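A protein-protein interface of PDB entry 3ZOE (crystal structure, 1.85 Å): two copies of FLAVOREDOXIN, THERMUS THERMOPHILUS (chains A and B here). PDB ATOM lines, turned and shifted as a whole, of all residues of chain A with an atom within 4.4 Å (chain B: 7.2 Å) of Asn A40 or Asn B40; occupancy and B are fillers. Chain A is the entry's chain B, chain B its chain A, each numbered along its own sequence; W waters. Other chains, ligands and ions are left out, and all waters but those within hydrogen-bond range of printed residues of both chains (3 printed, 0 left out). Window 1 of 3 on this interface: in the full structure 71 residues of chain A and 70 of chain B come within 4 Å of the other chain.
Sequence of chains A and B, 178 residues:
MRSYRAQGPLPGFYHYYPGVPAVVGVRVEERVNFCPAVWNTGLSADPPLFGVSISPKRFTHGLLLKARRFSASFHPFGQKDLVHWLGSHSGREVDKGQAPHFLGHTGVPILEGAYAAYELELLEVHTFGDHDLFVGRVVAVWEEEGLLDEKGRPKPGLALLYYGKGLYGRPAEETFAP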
ATOM      1  N   VAL A  20      22.822  -5.449 -30.825  1.00  0.00           N
ATOM      2  CA  VAL A  20      24.024  -4.995 -30.196  1.00  0.00           C
ATOM      3  C   VAL A  20      23.927  -5.304 -28.699  1.00  0.00           C
ATOM      4  O   VAL A  20      22.950  -4.932 -28.035  1.00  0.00           O
ATOM      5  CB  VAL A  20      24.247  -3.493 -30.436  1.00  0.00           C
ATOM      6  CG1 VAL A  20      25.487  -3.044 -29.662  1.00  0.00           C
ATOM      7  CG2 VAL A  20      24.468  -3.213 -31.922  1.00  0.00           C
ATOM      8  N   PRO A  21      24.942  -5.989 -28.151  1.00  0.00           N
ATOM      9  CA  PRO A  21      24.875  -6.189 -26.715  1.00  0.00           C
ATOM     10  C   PRO A  21      25.483  -4.964 -26.018  1.00  0.00           C
ATOM     11  O   PRO A  21      26.641  -4.583 -26.300  1.00  0.00           O
ATOM     12  CB  PRO A  21      25.673  -7.463 -26.521  1.00  0.00           C
ATOM     13  CG  PRO A  21      26.700  -7.421 -27.598  1.00  0.00           C
ATOM     14  CD  PRO A  21      26.045  -6.750 -28.773  1.00  0.00           C
ATOM     15  N   ALA A  22      24.713  -4.314 -25.162  1.00  0.00           N
ATOM     16  CA  ALA A  22      25.240  -3.217 -24.383  1.00  0.00           C
ATOM     17  C   ALA A  22      25.988  -3.768 -23.179  1.00  0.00           C
ATOM     18  O   ALA A  22      25.434  -4.511 -22.345  1.00  0.00           O
ATOM     19  CB  ALA A  22      24.110  -2.299 -23.932  1.00  0.00           C
ATOM     20  N   ALA A  37      24.262  -6.903 -21.943  1.00  0.00           N
ATOM     21  CA  ALA A  37      22.825  -7.056 -22.014  1.00  0.00           C
ATOM     22  C   ALA A  37      22.390  -6.879 -23.444  1.00  0.00           C
ATOM     23  O   ALA A  37      22.437  -5.779 -24.001  1.00  0.00           O
ATOM     24  CB  ALA A  37      22.134  -6.069 -21.071  1.00  0.00           C
ATOM     25  N   VAL A  38      21.896  -7.937 -24.066  1.00  0.00           N
ATOM     26  CA  VAL A  38      21.417  -7.752 -25.424  1.00  0.00           C
ATOM     27  C   VAL A  38      19.978  -7.250 -25.427  1.00  0.00           C
ATOM     28  O   VAL A  38      19.465  -6.750 -26.487  1.00  0.00           O
ATOM     29  CB  VAL A  38      21.627  -9.034 -26.293  1.00  0.00           C
ATOM     30  CG1 VAL A  38      20.770 -10.148 -25.861  1.00  0.00           C
ATOM     31  CG2 VAL A  38      21.380  -8.779 -27.797  1.00  0.00           C
ATOM     32  N   TRP A  39      19.305  -7.335 -24.256  1.00  0.00           N
ATOM     33  CA  TRP A  39      17.962  -6.779 -24.181  1.00  0.00           C
ATOM     34  C   TRP A  39      18.104  -5.346 -23.748  1.00  0.00           C
ATOM     35  O   TRP A  39      18.095  -5.033 -22.509  1.00  0.00           O
ATOM     36  CB  TRP A  39      17.044  -7.549 -23.213  1.00  0.00           C
ATOM     37  CG  TRP A  39      16.647  -8.852 -23.673  1.00  0.00           C
ATOM     38  CD1 TRP A  39      17.022  -9.451 -24.830  1.00  0.00           C
ATOM     39  CD2 TRP A  39      15.897  -9.836 -22.936  1.00  0.00           C
ATOM     40  NE1 TRP A  39      16.456 -10.695 -24.916  1.00  0.00           N
ATOM     41  CE2 TRP A  39      15.808 -10.984 -23.748  1.00  0.00           C
ATOM     42  CE3 TRP A  39      15.256  -9.845 -21.685  1.00  0.00           C
ATOM     43  CZ2 TRP A  39      15.099 -12.104 -23.373  1.00  0.00           C
ATOM     44  CZ3 TRP A  39      14.562 -11.000 -21.306  1.00  0.00           C
ATOM     45  CH2 TRP A  39      14.486 -12.089 -22.118  1.00  0.00           C
ATOM     46  N   ASN A  40      18.288  -4.493 -24.774  1.00  0.00           N
ATOM     47  CA  ASN A  40      18.458  -3.104 -24.560  1.00  0.00           C
ATOM     48  C   ASN A  40      17.811  -2.301 -25.656  1.00  0.00           C
ATOM     49  O   ASN A  40      17.706  -2.758 -26.791  1.00  0.00           O
ATOM     50  CB  ASN A  40      19.926  -2.743 -24.442  1.00  0.00           C
ATOM     51  CG  ASN A  40      20.656  -2.853 -25.775  1.00  0.00           C
ATOM     52  OD1 ASN A  40      20.591  -1.934 -26.565  1.00  0.00           O
ATOM     53  ND2 ASN A  40      21.384  -3.968 -25.995  1.00  0.00           N
ATOM     54  N   THR A  41      17.480  -1.062 -25.344  1.00  0.00           N
ATOM     55  CA  THR A  41      16.750  -0.208 -26.332  1.00  0.00           C
ATOM     56  C   THR A  41      16.751   1.232 -25.843  1.00  0.00           C
ATOM     57  O   THR A  41      16.647   1.526 -24.617  1.00  0.00           O
ATOM     58  CB  THR A  41      15.256  -0.671 -26.523  1.00  0.00           C
ATOM     59  OG1 THR A  41      14.551   0.125 -27.505  1.00  0.00           O
ATOM     60  CG2 THR A  41      14.491  -0.548 -25.197  1.00  0.00           C
ATOM     61  N   PHE A  50      17.578   5.380 -21.949  1.00  0.00           N
ATOM     62  CA  PHE A  50      18.059   4.113 -22.451  1.00  0.00           C
ATOM     63  C   PHE A  50      17.854   3.025 -21.397  1.00  0.00           C
ATOM     64  O   PHE A  50      18.032   3.226 -20.182  1.00  0.00           O
ATOM     65  CB  PHE A  50      19.536   4.276 -22.840  1.00  0.00           C
ATOM     66  CG  PHE A  50      20.142   3.059 -23.432  1.00  0.00           C
ATOM     67  CD1 PHE A  50      20.088   2.845 -24.769  1.00  0.00           C
ATOM     68  CD2 PHE A  50      20.838   2.149 -22.642  1.00  0.00           C
ATOM     69  CE1 PHE A  50      20.596   1.685 -25.332  1.00  0.00           C
ATOM     70  CE2 PHE A  50      21.414   1.026 -23.219  1.00  0.00           C
ATOM     71  CZ  PHE A  50      21.313   0.794 -24.548  1.00  0.00           C
ATOM     72  N   GLY A  51      17.406   1.873 -21.851  1.00  0.00           N
ATOM     73  CA  GLY A  51      17.031   0.807 -20.969  1.00  0.00           C
ATOM     74  C   GLY A  51      17.792  -0.467 -21.251  1.00  0.00           C
ATOM     75  O   GLY A  51      18.058  -0.790 -22.402  1.00  0.00           O
ATOM     76  N   VAL A  52      18.095  -1.167 -20.163  1.00  0.00           N
ATOM     77  CA  VAL A  52      18.668  -2.500 -20.107  1.00  0.00           C
ATOM     78  C   VAL A  52      17.787  -3.426 -19.262  1.00  0.00           C
ATOM     79  O   VAL A  52      17.297  -3.039 -18.184  1.00  0.00           O
ATOM     80  CB  VAL A  52      20.142  -2.419 -19.650  1.00  0.00           C
ATOM     81  CG1 VAL A  52      20.926  -1.536 -20.615  1.00  0.00           C
ATOM     82  CG2 VAL A  52      20.297  -1.847 -18.237  1.00  0.00           C
ATOM     83  N   TYR B  16      24.043   3.015 -30.022  1.00  0.00           N
ATOM     84  CA  TYR B  16      23.685   1.623 -29.767  1.00  0.00           C
ATOM     85  C   TYR B  16      23.090   0.892 -30.997  1.00  0.00           C
ATOM     86  O   TYR B  16      22.613  -0.274 -30.900  1.00  0.00           O
ATOM     87  CB  TYR B  16      22.726   1.566 -28.550  1.00  0.00           C
ATOM     88  CG  TYR B  16      21.514   2.451 -28.693  1.00  0.00           C
ATOM     89  CD1 TYR B  16      21.570   3.779 -28.330  1.00  0.00           C
ATOM     90  CD2 TYR B  16      20.324   1.971 -29.231  1.00  0.00           C
ATOM     91  CE1 TYR B  16      20.488   4.616 -28.473  1.00  0.00           C
ATOM     92  CE2 TYR B  16      19.226   2.800 -29.361  1.00  0.00           C
ATOM     93  CZ  TYR B  16      19.316   4.127 -28.969  1.00  0.00           C
ATOM     94  OH  TYR B  16      18.264   5.013 -29.107  1.00  0.00           O
ATOM     95  N   TYR B  17      23.114   1.567 -32.145  1.00  0.00           N
ATOM     96  CA  TYR B  17      22.626   0.996 -33.383  1.00  0.00           C
ATOM     97  C   TYR B  17      23.771   0.200 -34.004  1.00  0.00           C
ATOM     98  O   TYR B  17      24.975   0.393 -33.664  1.00  0.00           O
ATOM     99  CB  TYR B  17      22.137   2.082 -34.351  1.00  0.00           C
ATOM    100  CG  TYR B  17      20.797   2.756 -33.983  1.00  0.00           C
ATOM    101  CD1 TYR B  17      20.622   3.376 -32.778  1.00  0.00           C
ATOM    102  CD2 TYR B  17      19.769   2.825 -34.896  1.00  0.00           C
ATOM    103  CE1 TYR B  17      19.428   3.997 -32.465  1.00  0.00           C
ATOM    104  CE2 TYR B  17      18.594   3.459 -34.621  1.00  0.00           C
ATOM    105  CZ  TYR B  17      18.412   4.025 -33.401  1.00  0.00           C
ATOM    106  OH  TYR B  17      17.230   4.637 -33.127  1.00  0.00           O
ATOM    107  N   GLY B  19      20.036  -1.935 -35.070  1.00  0.00           N
ATOM    108  CA  GLY B  19      19.168  -2.956 -34.530  1.00  0.00           C
ATOM    109  C   GLY B  19      18.142  -3.418 -35.564  1.00  0.00           C
ATOM    110  O   GLY B  19      17.992  -2.800 -36.631  1.00  0.00           O
ATOM    111  N   VAL B  20      17.435  -4.502 -35.216  1.00  0.00           N
ATOM    112  CA  VAL B  20      16.398  -5.007 -36.026  1.00  0.00           C
ATOM    113  C   VAL B  20      15.145  -4.163 -35.772  1.00  0.00           C
ATOM    114  O   VAL B  20      14.763  -3.970 -34.607  1.00  0.00           O
ATOM    115  CB  VAL B  20      16.119  -6.504 -35.769  1.00  0.00           C
ATOM    116  CG1 VAL B  20      14.884  -6.944 -36.569  1.00  0.00           C
ATOM    117  CG2 VAL B  20      17.339  -7.345 -36.172  1.00  0.00           C
ATOM    118  N   PRO B  21      14.538  -3.637 -36.847  1.00  0.00           N
ATOM    119  CA  PRO B  21      13.280  -2.953 -36.707  1.00  0.00           C
ATOM    120  C   PRO B  21      12.152  -3.979 -36.685  1.00  0.00           C
ATOM    121  O   PRO B  21      12.054  -4.855 -37.549  1.00  0.00           O
ATOM    122  CB  PRO B  21      13.202  -2.059 -37.944  1.00  0.00           C
ATOM    123  CG  PRO B  21      14.338  -2.346 -38.784  1.00  0.00           C
ATOM    124  CD  PRO B  21      15.057  -3.535 -38.225  1.00  0.00           C
ATOM    125  N   ALA B  22      11.353  -3.925 -35.653  1.00  0.00           N
ATOM    126  CA  ALA B  22      10.170  -4.735 -35.581  1.00  0.00           C
ATOM    127  C   ALA B  22       9.105  -4.000 -36.348  1.00  0.00           C
ATOM    128  O   ALA B  22       8.836  -2.842 -36.036  1.00  0.00           O
ATOM    129  CB  ALA B  22       9.746  -4.911 -34.119  1.00  0.00           C
ATOM    130  N   VAL B  23       8.484  -4.641 -37.331  1.00  0.00           N
ATOM    131  CA  VAL B  23       7.219  -4.134 -37.860  1.00  0.00           C
ATOM    132  C   VAL B  23       5.976  -4.436 -36.978  1.00  0.00           C
ATOM    133  O   VAL B  23       5.614  -5.575 -36.675  1.00  0.00           O
ATOM    134  CB  VAL B  23       6.948  -4.540 -39.309  1.00  0.00           C
ATOM    135  CG1 VAL B  23       5.609  -3.951 -39.715  1.00  0.00           C
ATOM    136  CG2 VAL B  23       8.096  -4.054 -40.172  1.00  0.00           C
ATOM    137  N   VAL B  24       5.372  -3.351 -36.526  1.00  0.00           N
ATOM    138  CA  VAL B  24       4.307  -3.413 -35.524  1.00  0.00           C
ATOM    139  C   VAL B  24       2.991  -3.311 -36.314  1.00  0.00           C
ATOM    140  O   VAL B  24       2.708  -2.260 -36.905  1.00  0.00           O
ATOM    141  CB  VAL B  24       4.421  -2.276 -34.489  1.00  0.00           C
ATOM    142  CG1 VAL B  24       3.208  -2.246 -33.549  1.00  0.00           C
ATOM    143  CG2 VAL B  24       5.672  -2.449 -33.633  1.00  0.00           C
ATOM    144  N   ALA B  37       9.436  -0.250 -35.708  1.00  0.00           N
ATOM    145  CA  ALA B  37       9.956   0.224 -34.428  1.00  0.00           C
ATOM    146  C   ALA B  37      11.329  -0.364 -34.160  1.00  0.00           C
ATOM    147  O   ALA B  37      11.452  -1.554 -33.828  1.00  0.00           O
ATOM    148  CB  ALA B  37       8.980  -0.087 -33.287  1.00  0.00           C
ATOM    149  N   VAL B  38      12.380   0.444 -34.314  1.00  0.00           N
ATOM    150  CA  VAL B  38      13.702  -0.041 -33.981  1.00  0.00           C
ATOM    151  C   VAL B  38      14.004  -0.010 -32.472  1.00  0.00           C
ATOM    152  O   VAL B  38      14.923  -0.704 -32.010  1.00  0.00           O
ATOM    153  CB  VAL B  38      14.823   0.675 -34.753  1.00  0.00           C
ATOM    154  CG1 VAL B  38      14.956   2.112 -34.292  1.00  0.00           C
ATOM    155  CG2 VAL B  38      16.135  -0.102 -34.629  1.00  0.00           C
ATOM    156  N   TRP B  39      13.206   0.740 -31.703  1.00  0.00           N
ATOM    157  CA  TRP B  39      13.319   0.648 -30.258  1.00  0.00           C
ATOM    158  C   TRP B  39      12.429  -0.513 -29.834  1.00  0.00           C
ATOM    159  O   TRP B  39      11.238  -0.333 -29.560  1.00  0.00           O
ATOM    160  CB  TRP B  39      12.927   1.926 -29.547  1.00  0.00           C
ATOM    161  CG  TRP B  39      13.876   3.085 -29.776  1.00  0.00           C
ATOM    162  CD1 TRP B  39      15.046   3.078 -30.499  1.00  0.00           C
ATOM    163  CD2 TRP B  39      13.653   4.420 -29.390  1.00  0.00           C
ATOM    164  NE1 TRP B  39      15.599   4.330 -30.506  1.00  0.00           N
ATOM    165  CE2 TRP B  39      14.774   5.167 -29.793  1.00  0.00           C
ATOM    166  CE3 TRP B  39      12.673   5.049 -28.602  1.00  0.00           C
ATOM    167  CZ2 TRP B  39      14.906   6.531 -29.495  1.00  0.00           C
ATOM    168  CZ3 TRP B  39      12.805   6.399 -28.320  1.00  0.00           C
ATOM    169  CH2 TRP B  39      13.892   7.130 -28.785  1.00  0.00           C
ATOM    170  N   ASN B  40      13.010  -1.719 -29.850  1.00  0.00           N
ATOM    171  CA  ASN B  40      12.321  -2.884 -29.454  1.00  0.00           C
ATOM    172  C   ASN B  40      13.312  -3.734 -28.674  1.00  0.00           C
ATOM    173  O   ASN B  40      14.505  -3.541 -28.827  1.00  0.00           O
ATOM    174  CB  ASN B  40      11.724  -3.613 -30.654  1.00  0.00           C
ATOM    175  CG  ASN B  40      12.771  -4.338 -31.502  1.00  0.00           C
ATOM    176  OD1 ASN B  40      13.185  -5.444 -31.178  1.00  0.00           O
ATOM    177  ND2 ASN B  40      13.149  -3.727 -32.594  1.00  0.00           N
ATOM    178  N   THR B  41      12.801  -4.702 -27.925  1.00  0.00           N
ATOM    179  CA  THR B  41      13.664  -5.604 -27.145  1.00  0.00           C
ATOM    180  C   THR B  41      12.851  -6.667 -26.468  1.00  0.00           C
ATOM    181  O   THR B  41      11.667  -6.455 -26.067  1.00  0.00           O
ATOM    182  CB  THR B  41      14.414  -4.828 -26.022  1.00  0.00           C
ATOM    183  OG1 THR B  41      15.241  -5.751 -25.303  1.00  0.00           O
ATOM    184  CG2 THR B  41      13.421  -4.174 -25.007  1.00  0.00           C
ATOM    185  N   GLY B  42      13.467  -7.832 -26.280  1.00  0.00           N
ATOM    186  CA  GLY B  42      12.908  -8.828 -25.369  1.00  0.00           C
ATOM    187  C   GLY B  42      12.814  -8.243 -23.969  1.00  0.00           C
ATOM    188  O   GLY B  42      13.604  -7.406 -23.610  1.00  0.00           O
ATOM    189  N   LEU B  43      11.835  -8.665 -23.195  1.00  0.00           N
ATOM    190  CA  LEU B  43      11.761  -8.231 -21.789  1.00  0.00           C
ATOM    191  C   LEU B  43      11.583  -9.354 -20.763  1.00  0.00           C
ATOM    192  O   LEU B  43      11.772  -9.108 -19.605  1.00  0.00           O
ATOM    193  CB  LEU B  43      10.698  -7.192 -21.644  1.00  0.00           C
ATOM    194  CG  LEU B  43      10.972  -5.821 -22.324  1.00  0.00           C
ATOM    195  CD1 LEU B  43       9.627  -5.188 -22.609  1.00  0.00           C
ATOM    196  CD2 LEU B  43      11.804  -4.923 -21.422  1.00  0.00           C
ATOM    197  N   PHE B  50       7.659  -9.041 -24.983  1.00  0.00           N
ATOM    198  CA  PHE B  50       8.377  -8.298 -25.971  1.00  0.00           C
ATOM    199  C   PHE B  50       7.818  -6.897 -26.008  1.00  0.00           C
ATOM    200  O   PHE B  50       6.576  -6.672 -25.930  1.00  0.00           O
ATOM    201  CB  PHE B  50       8.287  -9.061 -27.337  1.00  0.00           C
ATOM    202  CG  PHE B  50       8.989  -8.366 -28.428  1.00  0.00           C
ATOM    203  CD1 PHE B  50      10.343  -8.545 -28.591  1.00  0.00           C
ATOM    204  CD2 PHE B  50       8.290  -7.537 -29.312  1.00  0.00           C
ATOM    205  CE1 PHE B  50      11.020  -7.899 -29.609  1.00  0.00           C
ATOM    206  CE2 PHE B  50       8.963  -6.899 -30.371  1.00  0.00           C
ATOM    207  CZ  PHE B  50      10.326  -7.100 -30.515  1.00  0.00           C
ATOM    208  N   GLY B  51       8.720  -5.943 -26.080  1.00  0.00           N
ATOM    209  CA  GLY B  51       8.367  -4.549 -25.953  1.00  0.00           C
ATOM    210  C   GLY B  51       8.718  -3.723 -27.161  1.00  0.00           C
ATOM    211  O   GLY B  51       9.772  -3.910 -27.801  1.00  0.00           O
ATOM    212  N   VAL B  52       7.826  -2.791 -27.475  1.00  0.00           N
ATOM    213  CA  VAL B  52       8.087  -1.806 -28.516  1.00  0.00           C
ATOM    214  C   VAL B  52       7.811  -0.411 -27.994  1.00  0.00           C
ATOM    215  O   VAL B  52       6.829  -0.187 -27.256  1.00  0.00           O
ATOM    216  CB  VAL B  52       7.279  -2.098 -29.794  1.00  0.00           C
ATOM    217  CG1 VAL B  52       7.617  -3.440 -30.410  1.00  0.00           C
ATOM    218  CG2 VAL B  52       5.755  -2.049 -29.515  1.00  0.00           C
ATOM    219  N   SER B  53       8.708   0.523 -28.338  1.00  0.00           N
ATOM    220  CA  SER B  53       8.624   1.851 -27.809  1.00  0.00           C
ATOM    221  C   SER B  53       8.151   2.784 -28.916  1.00  0.00           C
ATOM    222  O   SER B  53       8.825   2.932 -29.925  1.00  0.00           O
ATOM    223  CB  SER B  53       9.972   2.318 -27.246  1.00  0.00           C
ATOM    224  OG  SER B  53       9.894   3.632 -26.685  1.00  0.00           O
ATOM    225  N   ALA B  72       4.255  -8.195 -33.976  1.00  0.00           N
ATOM    226  CA  ALA B  72       5.623  -7.729 -34.273  1.00  0.00           C
ATOM    227  C   ALA B  72       6.248  -8.726 -35.235  1.00  0.00           C
ATOM    228  O   ALA B  72       6.380  -9.908 -34.915  1.00  0.00           O
ATOM    229  CB  ALA B  72       6.429  -7.571 -33.012  1.00  0.00           C
ATOM    230  N   PHE B  74       9.378  -9.565 -38.359  1.00  0.00           N
ATOM    231  CA  PHE B  74      10.794  -9.378 -38.558  1.00  0.00           C
ATOM    232  C   PHE B  74      11.134  -9.781 -40.002  1.00  0.00           C
ATOM    233  O   PHE B  74      10.922 -10.934 -40.442  1.00  0.00           O
ATOM    234  CB  PHE B  74      11.570 -10.164 -37.471  1.00  0.00           C
ATOM    235  CG  PHE B  74      11.088  -9.891 -36.065  1.00  0.00           C
ATOM    236  CD1 PHE B  74      11.310  -8.678 -35.475  1.00  0.00           C
ATOM    237  CD2 PHE B  74      10.363 -10.841 -35.346  1.00  0.00           C
ATOM    238  CE1 PHE B  74      10.819  -8.398 -34.200  1.00  0.00           C
ATOM    239  CE2 PHE B  74       9.853 -10.579 -34.068  1.00  0.00           C
ATOM    240  CZ  PHE B  74      10.118  -9.353 -33.485  1.00  0.00           C
ATOM    241  N   LEU B 133       6.482   2.725 -23.858  1.00  0.00           N
ATOM    242  CA  LEU B 133       6.832   1.335 -24.015  1.00  0.00           C
ATOM    243  C   LEU B 133       5.588   0.451 -23.908  1.00  0.00           C
ATOM    244  O   LEU B 133       4.921   0.407 -22.849  1.00  0.00           O
ATOM    245  CB  LEU B 133       7.887   0.917 -22.995  1.00  0.00           C
ATOM    246  CG  LEU B 133       8.319  -0.548 -23.154  1.00  0.00           C
ATOM    247  CD1 LEU B 133       9.095  -0.744 -24.474  1.00  0.00           C
ATOM    248  CD2 LEU B 133       9.187  -0.967 -21.962  1.00  0.00           C
HETATM  249  O   HOH W   1      16.587  -7.410 -27.802  1.00  0.00           O
HETATM  250  O   HOH W   2      17.134   0.326 -29.718  1.00  0.00           O
HETATM  251  O   HOH W   3      20.977  -1.714 -29.353  1.00  0.00           O
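Of chain B, only Asn B40 and Thr B41 come within 4 Å of Asn A40. Of the printed residues of chain A, Tyr B16 touches Val A20 (3.6 Å) and Phe A50 (3.6 Å). Val B20 touches none of the printed residues of chain A. Printed residues of chain A within 4 Å of Trp B39: Thr A41 (3.1 Å). Asn B40 touches just these residues of chain A: Asn A40 and Thr A41. Printed residues of chain A within 4 Å of Thr B41: Trp A39 (3.1 Å), Asn A40 (3.3 Å) and Thr A41 (3.8 Å). Of the printed residues of chain A, Gly B42 touches Trp A39. The nearest residue of chain B that does not touch Asn A40 is Tyr B16 (4.6 Å). The nearest printed residue of chain A that does not touch Asn B40 is Val A38 (6.4 Å). The nearest printed residue of chain B that does not touch Trp A39 is Asn B40 (6.5 Å).
Printed residues of chain A that touch a printed residue of chain B: Val A20, Trp A39, Asn A40, Thr A41 and Phe A50.
Trp A39 touches Thr B41, and with the chains exchanged Thr A41 touches Trp B39. Asn B40 touches its own counterpart, Asn A40. Asn A40 touches Thr B41, and with the chains exchanged Thr A41 touches Asn B40. Thr B41 touches its own counterpart, Thr A41.
Water W3 bridges the backbone carbonyl oxygen (O) of Tyr B16 (2.7 Å) and the side-chain amide oxygen (OD1) of Asn A40 (2.8 Å). Water W1 lies within hydrogen-bond range of the backbone carbonyl oxygen (O) of Val A38 (3.2 Å), the side-chain hydroxyl (OG1) of Thr B41 (3.3 Å) and the backbone NH (N) of Gly B42 (3.5 Å). Water W2 bridges the backbone carbonyl oxygen of Val B38 and the side-chain hydroxyl of Thr A41.
The backbone carbonyl oxygen (O) of Val A20 lies within hydrogen-bond range of the side-chain amide nitrogen (ND2) of Asn A40 (2.7 Å). The side-chain hydroxyl (OH) of Tyr B16 is in hydrogen-bond range of the indole nitrogen (NE1) of Trp B39, at 3.1 Å. O of Thr A41 lies within hydrogen-bond range of N of Gly A51, at 2.9 Å. The backbone carbonyl oxygen of Val B20 is in hydrogen-bond range of the side-chain amide nitrogen of Asn B40 (2.6 Å). The backbone NH of Ala A22 lies close to the side-chain amide nitrogen of Asn A40, 3.4 Å away. The side-chain amide nitrogen (ND2) of Asn A40 lies within hydrogen-bond range of the backbone carbonyl oxygen (O) of Val A38, 3.4 Å away.
The side-chain hydroxyl (OG1) of Thr A41 is in hydrogen-bond range of the backbone NH (N) of Asn B40 (3.4 Å). OG1 of Thr B41 sits at hydrogen-bond distance from N of Asn A40 (3.3 Å).
Among the printed residues, pairs that only touch across the chains: Thr A41 with Trp B39, Trp A39 with Thr B41, Trp A39 with Gly B42, Trp A39 with Leu B43, Phe A50 with Tyr B16, Val A20 with Tyr B16, Thr A41 with Thr B41 and Asn A40 with Asn B40.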
